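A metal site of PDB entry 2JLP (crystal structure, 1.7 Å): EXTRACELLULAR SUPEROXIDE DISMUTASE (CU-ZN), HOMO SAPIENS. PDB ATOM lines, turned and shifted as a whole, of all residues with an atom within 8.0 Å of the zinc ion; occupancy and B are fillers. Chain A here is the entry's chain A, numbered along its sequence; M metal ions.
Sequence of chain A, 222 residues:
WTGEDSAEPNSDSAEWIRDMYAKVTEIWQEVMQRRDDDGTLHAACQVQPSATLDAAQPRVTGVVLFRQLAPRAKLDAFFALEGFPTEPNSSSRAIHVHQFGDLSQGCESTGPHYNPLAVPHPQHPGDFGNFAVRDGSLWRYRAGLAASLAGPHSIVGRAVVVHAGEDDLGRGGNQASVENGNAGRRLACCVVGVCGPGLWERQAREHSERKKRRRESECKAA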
ATOM      1  N   ILE A  95       3.282   4.055  12.577  1.00  0.00           N
ATOM      2  CA  ILE A  95       2.308   3.975  13.642  1.00  0.00           C
ATOM      3  C   ILE A  95       1.687   2.576  13.634  1.00  0.00           C
ATOM      4  O   ILE A  95       1.296   2.082  12.560  1.00  0.00           O
ATOM      5  CB  ILE A  95       1.213   5.025  13.508  1.00  0.00           C
ATOM      6  CG1 ILE A  95       1.868   6.443  13.433  1.00  0.00           C
ATOM      7  CG2 ILE A  95       0.257   4.886  14.671  1.00  0.00           C
ATOM      8  CD1 ILE A  95       0.895   7.625  13.196  1.00  0.00           C
ATOM      9  N   HIS A  96       1.613   1.961  14.815  1.00  0.00           N
ATOM     10  CA  HIS A  96       1.038   0.627  14.899  1.00  0.00           C
ATOM     11  C   HIS A  96       0.192   0.450  16.156  1.00  0.00           C
ATOM     12  O   HIS A  96       0.400   1.167  17.128  1.00  0.00           O
ATOM     13  CB  HIS A  96       2.138  -0.419  15.020  1.00  0.00           C
ATOM     14  CG  HIS A  96       3.326  -0.254  14.114  1.00  0.00           C
ATOM     15  ND1 HIS A  96       4.583  -0.058  14.620  1.00  0.00           N
ATOM     16  CD2 HIS A  96       3.463  -0.417  12.773  1.00  0.00           C
ATOM     17  CE1 HIS A  96       5.451  -0.060  13.623  1.00  0.00           C
ATOM     18  NE2 HIS A  96       4.804  -0.250  12.489  1.00  0.00           N
ATOM     19  N   VAL A  97      -0.503  -0.678  16.208  1.00  0.00           N
ATOM     20  CA  VAL A  97      -1.175  -1.108  17.434  1.00  0.00           C
ATOM     21  C   VAL A  97      -0.278  -2.151  18.125  1.00  0.00           C
ATOM     22  O   VAL A  97       0.133  -3.134  17.491  1.00  0.00           O
ATOM     23  CB  VAL A  97      -2.574  -1.730  17.173  1.00  0.00           C
ATOM     24  CG1 VAL A  97      -3.196  -2.201  18.451  1.00  0.00           C
ATOM     25  CG2 VAL A  97      -3.520  -0.769  16.409  1.00  0.00           C
ATOM     26  N   HIS A  98      -0.026  -1.942  19.411  1.00  0.00           N
ATOM     27  CA  HIS A  98       0.717  -2.813  20.293  1.00  0.00           C
ATOM     28  C   HIS A  98      -0.249  -3.493  21.264  1.00  0.00           C
ATOM     29  O   HIS A  98      -1.414  -3.011  21.515  1.00  0.00           O
ATOM     30  CB  HIS A  98       1.820  -2.070  21.009  1.00  0.00           C
ATOM     31  CG  HIS A  98       2.918  -1.674  20.101  1.00  0.00           C
ATOM     32  ND1 HIS A  98       4.230  -2.072  20.292  1.00  0.00           N
ATOM     33  CD2 HIS A  98       2.897  -0.966  18.944  1.00  0.00           C
ATOM     34  CE1 HIS A  98       4.969  -1.590  19.314  1.00  0.00           C
ATOM     35  NE2 HIS A  98       4.206  -0.911  18.499  1.00  0.00           N
ATOM     36  N   PRO A 112       4.596  -6.086  22.289  1.00  0.00           N
ATOM     37  CA  PRO A 112       4.891  -6.133  20.867  1.00  0.00           C
ATOM     38  C   PRO A 112       3.684  -5.785  20.026  1.00  0.00           C
ATOM     39  O   PRO A 112       2.636  -5.475  20.638  1.00  0.00           O
ATOM     40  CB  PRO A 112       5.212  -7.603  20.655  1.00  0.00           C
ATOM     41  CG  PRO A 112       4.376  -8.285  21.628  1.00  0.00           C
ATOM     42  CD  PRO A 112       4.296  -7.404  22.824  1.00  0.00           C
ATOM     43  N   HIS A 113       3.806  -5.857  18.688  1.00  0.00           N
ATOM     44  CA  HIS A 113       2.662  -5.526  17.816  1.00  0.00           C
ATOM     45  C   HIS A 113       1.555  -6.520  18.181  1.00  0.00           C
ATOM     46  O   HIS A 113       1.836  -7.708  18.424  1.00  0.00           O
ATOM     47  CB  HIS A 113       3.038  -5.641  16.343  1.00  0.00           C
ATOM     48  CG  HIS A 113       3.956  -4.566  15.884  1.00  0.00           C
ATOM     49  ND1 HIS A 113       4.170  -4.266  14.562  1.00  0.00           N
ATOM     50  CD2 HIS A 113       4.707  -3.682  16.614  1.00  0.00           C
ATOM     51  CE1 HIS A 113       5.025  -3.256  14.478  1.00  0.00           C
ATOM     52  NE2 HIS A 113       5.338  -2.859  15.709  1.00  0.00           N
ATOM     53  N   TYR A 114       0.303  -6.054  18.225  1.00  0.00           N
ATOM     54  CA  TYR A 114      -0.793  -6.931  18.555  1.00  0.00           C
ATOM     55  C   TYR A 114      -0.913  -7.969  17.431  1.00  0.00           C
ATOM     56  O   TYR A 114      -1.012  -7.628  16.264  1.00  0.00           O
ATOM     57  CB  TYR A 114      -2.083  -6.107  18.729  1.00  0.00           C
ATOM     58  CG  TYR A 114      -3.314  -6.942  18.942  1.00  0.00           C
ATOM     59  CD1 TYR A 114      -3.347  -7.950  19.900  1.00  0.00           C
ATOM     60  CD2 TYR A 114      -4.499  -6.702  18.210  1.00  0.00           C
ATOM     61  CE1 TYR A 114      -4.488  -8.664  20.134  1.00  0.00           C
ATOM     62  CE2 TYR A 114      -5.657  -7.429  18.435  1.00  0.00           C
ATOM     63  CZ  TYR A 114      -5.653  -8.415  19.396  1.00  0.00           C
ATOM     64  OH  TYR A 114      -6.767  -9.233  19.627  1.00  0.00           O
ATOM     65  N   ASN A 115      -0.971  -9.244  17.780  1.00  0.00           N
ATOM     66  CA  ASN A 115      -0.746 -10.283  16.813  1.00  0.00           C
ATOM     67  C   ASN A 115      -1.603 -11.530  17.118  1.00  0.00           C
ATOM     68  O   ASN A 115      -1.097 -12.636  17.362  1.00  0.00           O
ATOM     69  CB  ASN A 115       0.766 -10.590  16.740  1.00  0.00           C
ATOM     70  CG  ASN A 115       1.136 -11.531  15.592  1.00  0.00           C
ATOM     71  OD1 ASN A 115       0.338 -11.779  14.686  1.00  0.00           O
ATOM     72  ND2 ASN A 115       2.375 -12.014  15.608  1.00  0.00           N
ATOM     73  N   VAL A 119       1.188 -14.109  13.091  1.00  0.00           N
ATOM     74  CA  VAL A 119       1.751 -13.903  11.743  1.00  0.00           C
ATOM     75  C   VAL A 119       2.918 -12.891  11.798  1.00  0.00           C
ATOM     76  O   VAL A 119       3.006 -12.134  12.780  1.00  0.00           O
ATOM     77  CB  VAL A 119       0.637 -13.395  10.742  1.00  0.00           C
ATOM     78  CG1 VAL A 119      -0.452 -14.470  10.490  1.00  0.00           C
ATOM     79  CG2 VAL A 119       0.041 -12.080  11.179  1.00  0.00           C
ATOM     80  N   PRO A 120       3.773 -12.882  10.777  1.00  0.00           N
ATOM     81  CA  PRO A 120       4.847 -11.891  10.774  1.00  0.00           C
ATOM     82  C   PRO A 120       4.396 -10.500  10.414  1.00  0.00           C
ATOM     83  O   PRO A 120       3.351 -10.296   9.748  1.00  0.00           O
ATOM     84  CB  PRO A 120       5.829 -12.443   9.737  1.00  0.00           C
ATOM     85  CG  PRO A 120       4.986 -13.187   8.791  1.00  0.00           C
ATOM     86  CD  PRO A 120       3.901 -13.814   9.630  1.00  0.00           C
ATOM     87  N   HIS A 121       5.144  -9.507  10.887  1.00  0.00           N
ATOM     88  CA  HIS A 121       5.023  -8.181  10.364  1.00  0.00           C
ATOM     89  C   HIS A 121       5.331  -8.166   8.879  1.00  0.00           C
ATOM     90  O   HIS A 121       6.310  -8.838   8.429  1.00  0.00           O
ATOM     91  CB  HIS A 121       6.029  -7.265  11.092  1.00  0.00           C
ATOM     92  CG  HIS A 121       5.875  -5.804  10.776  1.00  0.00           C
ATOM     93  ND1 HIS A 121       4.948  -4.975  11.396  1.00  0.00           N
ATOM     94  CD2 HIS A 121       6.551  -5.034   9.895  1.00  0.00           C
ATOM     95  CE1 HIS A 121       5.056  -3.770  10.863  1.00  0.00           C
ATOM     96  NE2 HIS A 121       6.054  -3.761   9.987  1.00  0.00           N
ATOM     97  N   PRO A 122       4.564  -7.388   8.065  1.00  0.00           N
ATOM     98  CA  PRO A 122       3.518  -6.417   8.385  1.00  0.00           C
ATOM     99  C   PRO A 122       2.113  -6.920   8.198  1.00  0.00           C
ATOM    100  O   PRO A 122       1.238  -6.173   7.662  1.00  0.00           O
ATOM    101  CB  PRO A 122       3.824  -5.292   7.383  1.00  0.00           C
ATOM    102  CG  PRO A 122       4.176  -6.034   6.142  1.00  0.00           C
ATOM    103  CD  PRO A 122       4.842  -7.360   6.626  1.00  0.00           C
ATOM    104  N   GLN A 123       1.864  -8.183   8.595  1.00  0.00           N
ATOM    105  CA  GLN A 123       0.530  -8.776   8.523  1.00  0.00           C
ATOM    106  C   GLN A 123      -0.326  -8.580   9.778  1.00  0.00           C
ATOM    107  O   GLN A 123      -1.439  -9.075   9.855  1.00  0.00           O
ATOM    108  CB  GLN A 123       0.639 -10.265   8.146  1.00  0.00           C
ATOM    109  CG  GLN A 123       1.394 -10.568   6.869  1.00  0.00           C
ATOM    110  CD  GLN A 123       1.529 -12.088   6.661  1.00  0.00           C
ATOM    111  OE1 GLN A 123       0.621 -12.869   7.044  1.00  0.00           O
ATOM    112  NE2 GLN A 123       2.662 -12.515   6.108  1.00  0.00           N
ATOM    113  N   HIS A 124       0.164  -7.818  10.753  1.00  0.00           N
ATOM    114  CA  HIS A 124      -0.548  -7.643  12.019  1.00  0.00           C
ATOM    115  C   HIS A 124      -1.735  -6.687  11.718  1.00  0.00           C
ATOM    116  O   HIS A 124      -1.622  -5.814  10.873  1.00  0.00           O
ATOM    117  CB  HIS A 124       0.365  -7.020  13.078  1.00  0.00           C
ATOM    118  CG  HIS A 124       1.643  -7.744  13.330  1.00  0.00           C
ATOM    119  ND1 HIS A 124       2.839  -7.068  13.455  1.00  0.00           N
ATOM    120  CD2 HIS A 124       1.912  -9.072  13.449  1.00  0.00           C
ATOM    121  CE1 HIS A 124       3.795  -7.962  13.690  1.00  0.00           C
ATOM    122  NE2 HIS A 124       3.263  -9.182  13.694  1.00  0.00           N
ATOM    123  N   PRO A 125      -2.852  -6.833  12.445  1.00  0.00           N
ATOM    124  CA  PRO A 125      -4.029  -6.081  12.065  1.00  0.00           C
ATOM    125  C   PRO A 125      -3.868  -4.587  12.247  1.00  0.00           C
ATOM    126  O   PRO A 125      -4.465  -3.829  11.490  1.00  0.00           O
ATOM    127  CB  PRO A 125      -5.099  -6.624  12.998  1.00  0.00           C
ATOM    128  CG  PRO A 125      -4.386  -7.203  14.136  1.00  0.00           C
ATOM    129  CD  PRO A 125      -3.148  -7.775  13.542  1.00  0.00           C
ATOM    130  N   GLY A 126      -3.004  -4.207  13.193  1.00  0.00           N
ATOM    131  CA  GLY A 126      -2.715  -2.796  13.524  1.00  0.00           C
ATOM    132  C   GLY A 126      -1.469  -2.242  12.872  1.00  0.00           C
ATOM    133  O   GLY A 126      -0.966  -1.161  13.274  1.00  0.00           O
ATOM    134  N   ASP A 127      -0.953  -2.936  11.848  1.00  0.00           N
ATOM    135  CA  ASP A 127       0.157  -2.422  11.065  1.00  0.00           C
ATOM    136  C   ASP A 127      -0.312  -1.315  10.108  1.00  0.00           C
ATOM    137  O   ASP A 127      -0.557  -1.600   8.943  1.00  0.00           O
ATOM    138  CB  ASP A 127       0.837  -3.538  10.294  1.00  0.00           C
ATOM    139  CG  ASP A 127       1.632  -4.419  11.167  1.00  0.00           C
ATOM    140  OD1 ASP A 127       2.089  -3.947  12.257  1.00  0.00           O
ATOM    141  OD2 ASP A 127       1.860  -5.610  10.781  1.00  0.00           O
ATOM    142  N   PHE A 128      -0.367  -0.077  10.608  1.00  0.00           N
ATOM    143  CA  PHE A 128      -0.920   1.037   9.824  1.00  0.00           C
ATOM    144  C   PHE A 128       0.006   1.643   8.815  1.00  0.00           C
ATOM    145  O   PHE A 128      -0.464   2.390   7.958  1.00  0.00           O
ATOM    146  CB  PHE A 128      -1.402   2.146  10.719  1.00  0.00           C
ATOM    147  CG  PHE A 128      -2.476   1.719  11.733  1.00  0.00           C
ATOM    148  CD1 PHE A 128      -3.367   0.710  11.454  1.00  0.00           C
ATOM    149  CD2 PHE A 128      -2.620   2.425  12.918  1.00  0.00           C
ATOM    150  CE1 PHE A 128      -4.368   0.382  12.341  1.00  0.00           C
ATOM    151  CE2 PHE A 128      -3.568   2.037  13.845  1.00  0.00           C
ATOM    152  CZ  PHE A 128      -4.454   1.060  13.529  1.00  0.00           C
ATOM    153  N   ASP A 167       8.908   2.324   8.825  1.00  0.00           N
ATOM    154  CA  ASP A 167       8.595   0.916   8.829  1.00  0.00           C
ATOM    155  C   ASP A 167       9.100   0.351   7.490  1.00  0.00           C
ATOM    156  O   ASP A 167       8.716   0.807   6.398  1.00  0.00           O
ATOM    157  CB  ASP A 167       7.068   0.787   8.887  1.00  0.00           C
ATOM    158  CG  ASP A 167       6.581  -0.633   9.192  1.00  0.00           C
ATOM    159  OD1 ASP A 167       7.149  -1.610   8.709  1.00  0.00           O
ATOM    160  OD2 ASP A 167       5.603  -0.745   9.934  1.00  0.00           O
ATOM    161  N   ALA A 176      14.207  -8.168  13.251  1.00  0.00           N
ATOM    162  CA  ALA A 176      13.321  -7.095  13.595  1.00  0.00           C
ATOM    163  C   ALA A 176      12.401  -6.662  12.440  1.00  0.00           C
ATOM    164  O   ALA A 176      11.283  -6.246  12.658  1.00  0.00           O
ATOM    165  CB  ALA A 176      14.112  -5.886  14.038  1.00  0.00           C
ATOM    166  N   SER A 177      12.903  -6.709  11.214  1.00  0.00           N
ATOM    167  CA  SER A 177      12.081  -6.302  10.091  1.00  0.00           C
ATOM    168  C   SER A 177      10.714  -7.031  10.096  1.00  0.00           C
ATOM    169  O   SER A 177       9.665  -6.384   9.830  1.00  0.00           O
ATOM    170  CB  SER A 177      12.823  -6.498   8.798  1.00  0.00           C
ATOM    171  OG  SER A 177      12.001  -6.055   7.730  1.00  0.00           O
ATOM    172  N   VAL A 178      10.754  -8.347  10.359  1.00  0.00           N
ATOM    173  CA  VAL A 178       9.562  -9.189  10.399  1.00  0.00           C
ATOM    174  C   VAL A 178       8.820  -9.278  11.765  1.00  0.00           C
ATOM    175  O   VAL A 178       7.849 -10.071  11.942  1.00  0.00           O
ATOM    176  CB  VAL A 178       9.845 -10.585   9.773  1.00  0.00           C
ATOM    177  CG1 VAL A 178      10.162 -10.425   8.266  1.00  0.00           C
ATOM    178  CG2 VAL A 178      10.940 -11.364  10.494  1.00  0.00           C
ATOM    179  N   GLU A 179       9.272  -8.435  12.724  1.00  0.00           N
ATOM    180  CA  GLU A 179       8.596  -8.254  14.011  1.00  0.00           C
ATOM    181  C   GLU A 179       7.953  -6.881  14.081  1.00  0.00           C
ATOM    182  O   GLU A 179       6.815  -6.766  14.500  1.00  0.00           O
ATOM    183  CB  GLU A 179       9.590  -8.468  15.169  1.00  0.00           C
ATOM    184  CG  GLU A 179      10.230  -9.836  15.116  1.00  0.00           C
ATOM    185  CD  GLU A 179       9.273 -10.985  15.436  1.00  0.00           C
ATOM    186  OE1 GLU A 179       8.229 -10.752  16.046  1.00  0.00           O
ATOM    187  OE2 GLU A 179       9.573 -12.119  15.050  1.00  0.00           O
ATOM    188  N   ASN A 180       8.711  -5.835  13.708  1.00  0.00           N
ATOM    189  CA  ASN A 180       8.270  -4.452  13.883  1.00  0.00           C
ATOM    190  C   ASN A 180       8.703  -3.513  12.784  1.00  0.00           C
ATOM    191  O   ASN A 180       8.501  -2.324  12.895  1.00  0.00           O
ATOM    192  CB  ASN A 180       8.769  -3.911  15.217  1.00  0.00           C
ATOM    193  CG  ASN A 180      10.259  -3.986  15.378  1.00  0.00           C
ATOM    194  OD1 ASN A 180      11.056  -3.693  14.463  1.00  0.00           O
ATOM    195  ND2 ASN A 180      10.683  -4.352  16.591  1.00  0.00           N
ATOM    196  N   GLY A 181       9.320  -4.034  11.714  1.00  0.00           N
ATOM    197  CA  GLY A 181       9.632  -3.218  10.560  1.00  0.00           C
ATOM    198  C   GLY A 181      10.787  -2.282  10.784  1.00  0.00           C
ATOM    199  O   GLY A 181      10.998  -1.370   9.942  1.00  0.00           O
HETATM  200 ZN    ZN M   1       3.505  -5.259  12.954  1.00  0.00          ZN
HETATM  201 CU    CU M   2       4.734   0.036  16.784  1.00  0.00          CU
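The zinc ion is bound by ND1 of His 124 (2.0 Å), ND1 of His 113 (2.0 Å), OD1 of Asp 127 (2.1 Å) and ND1 of His 121 (2.1 Å).
The zinc ion has four donor atoms within binding distance.
Slightly farther from the zinc ion lies OD2 of Asp 127 (2.7 Å).
The backbone carbonyl oxygen of Val 178 lies within hydrogen-bond range of the backbone NH of His 121 (3.0 Å).
A ring nitrogen (NE2) of His 124 is in hydrogen-bond range of the backbone carbonyl oxygen (O) of Val 119, at 3.1 Å.
NE2 of His 121 lies within hydrogen-bond range of OD1 of Asp 167.
The backbone NH (N) of Gln 123 sits at hydrogen-bond distance from the side-chain carboxylate (OD2) of Asp 127 (3.4 Å).
ND1 of His 96 sits close to NE2 of His 113 (3.1 Å).
Glu 179 touches the zinc ion.
The nearest printed residue that does not touch the zinc ion is Pro 122 (4.7 Å).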
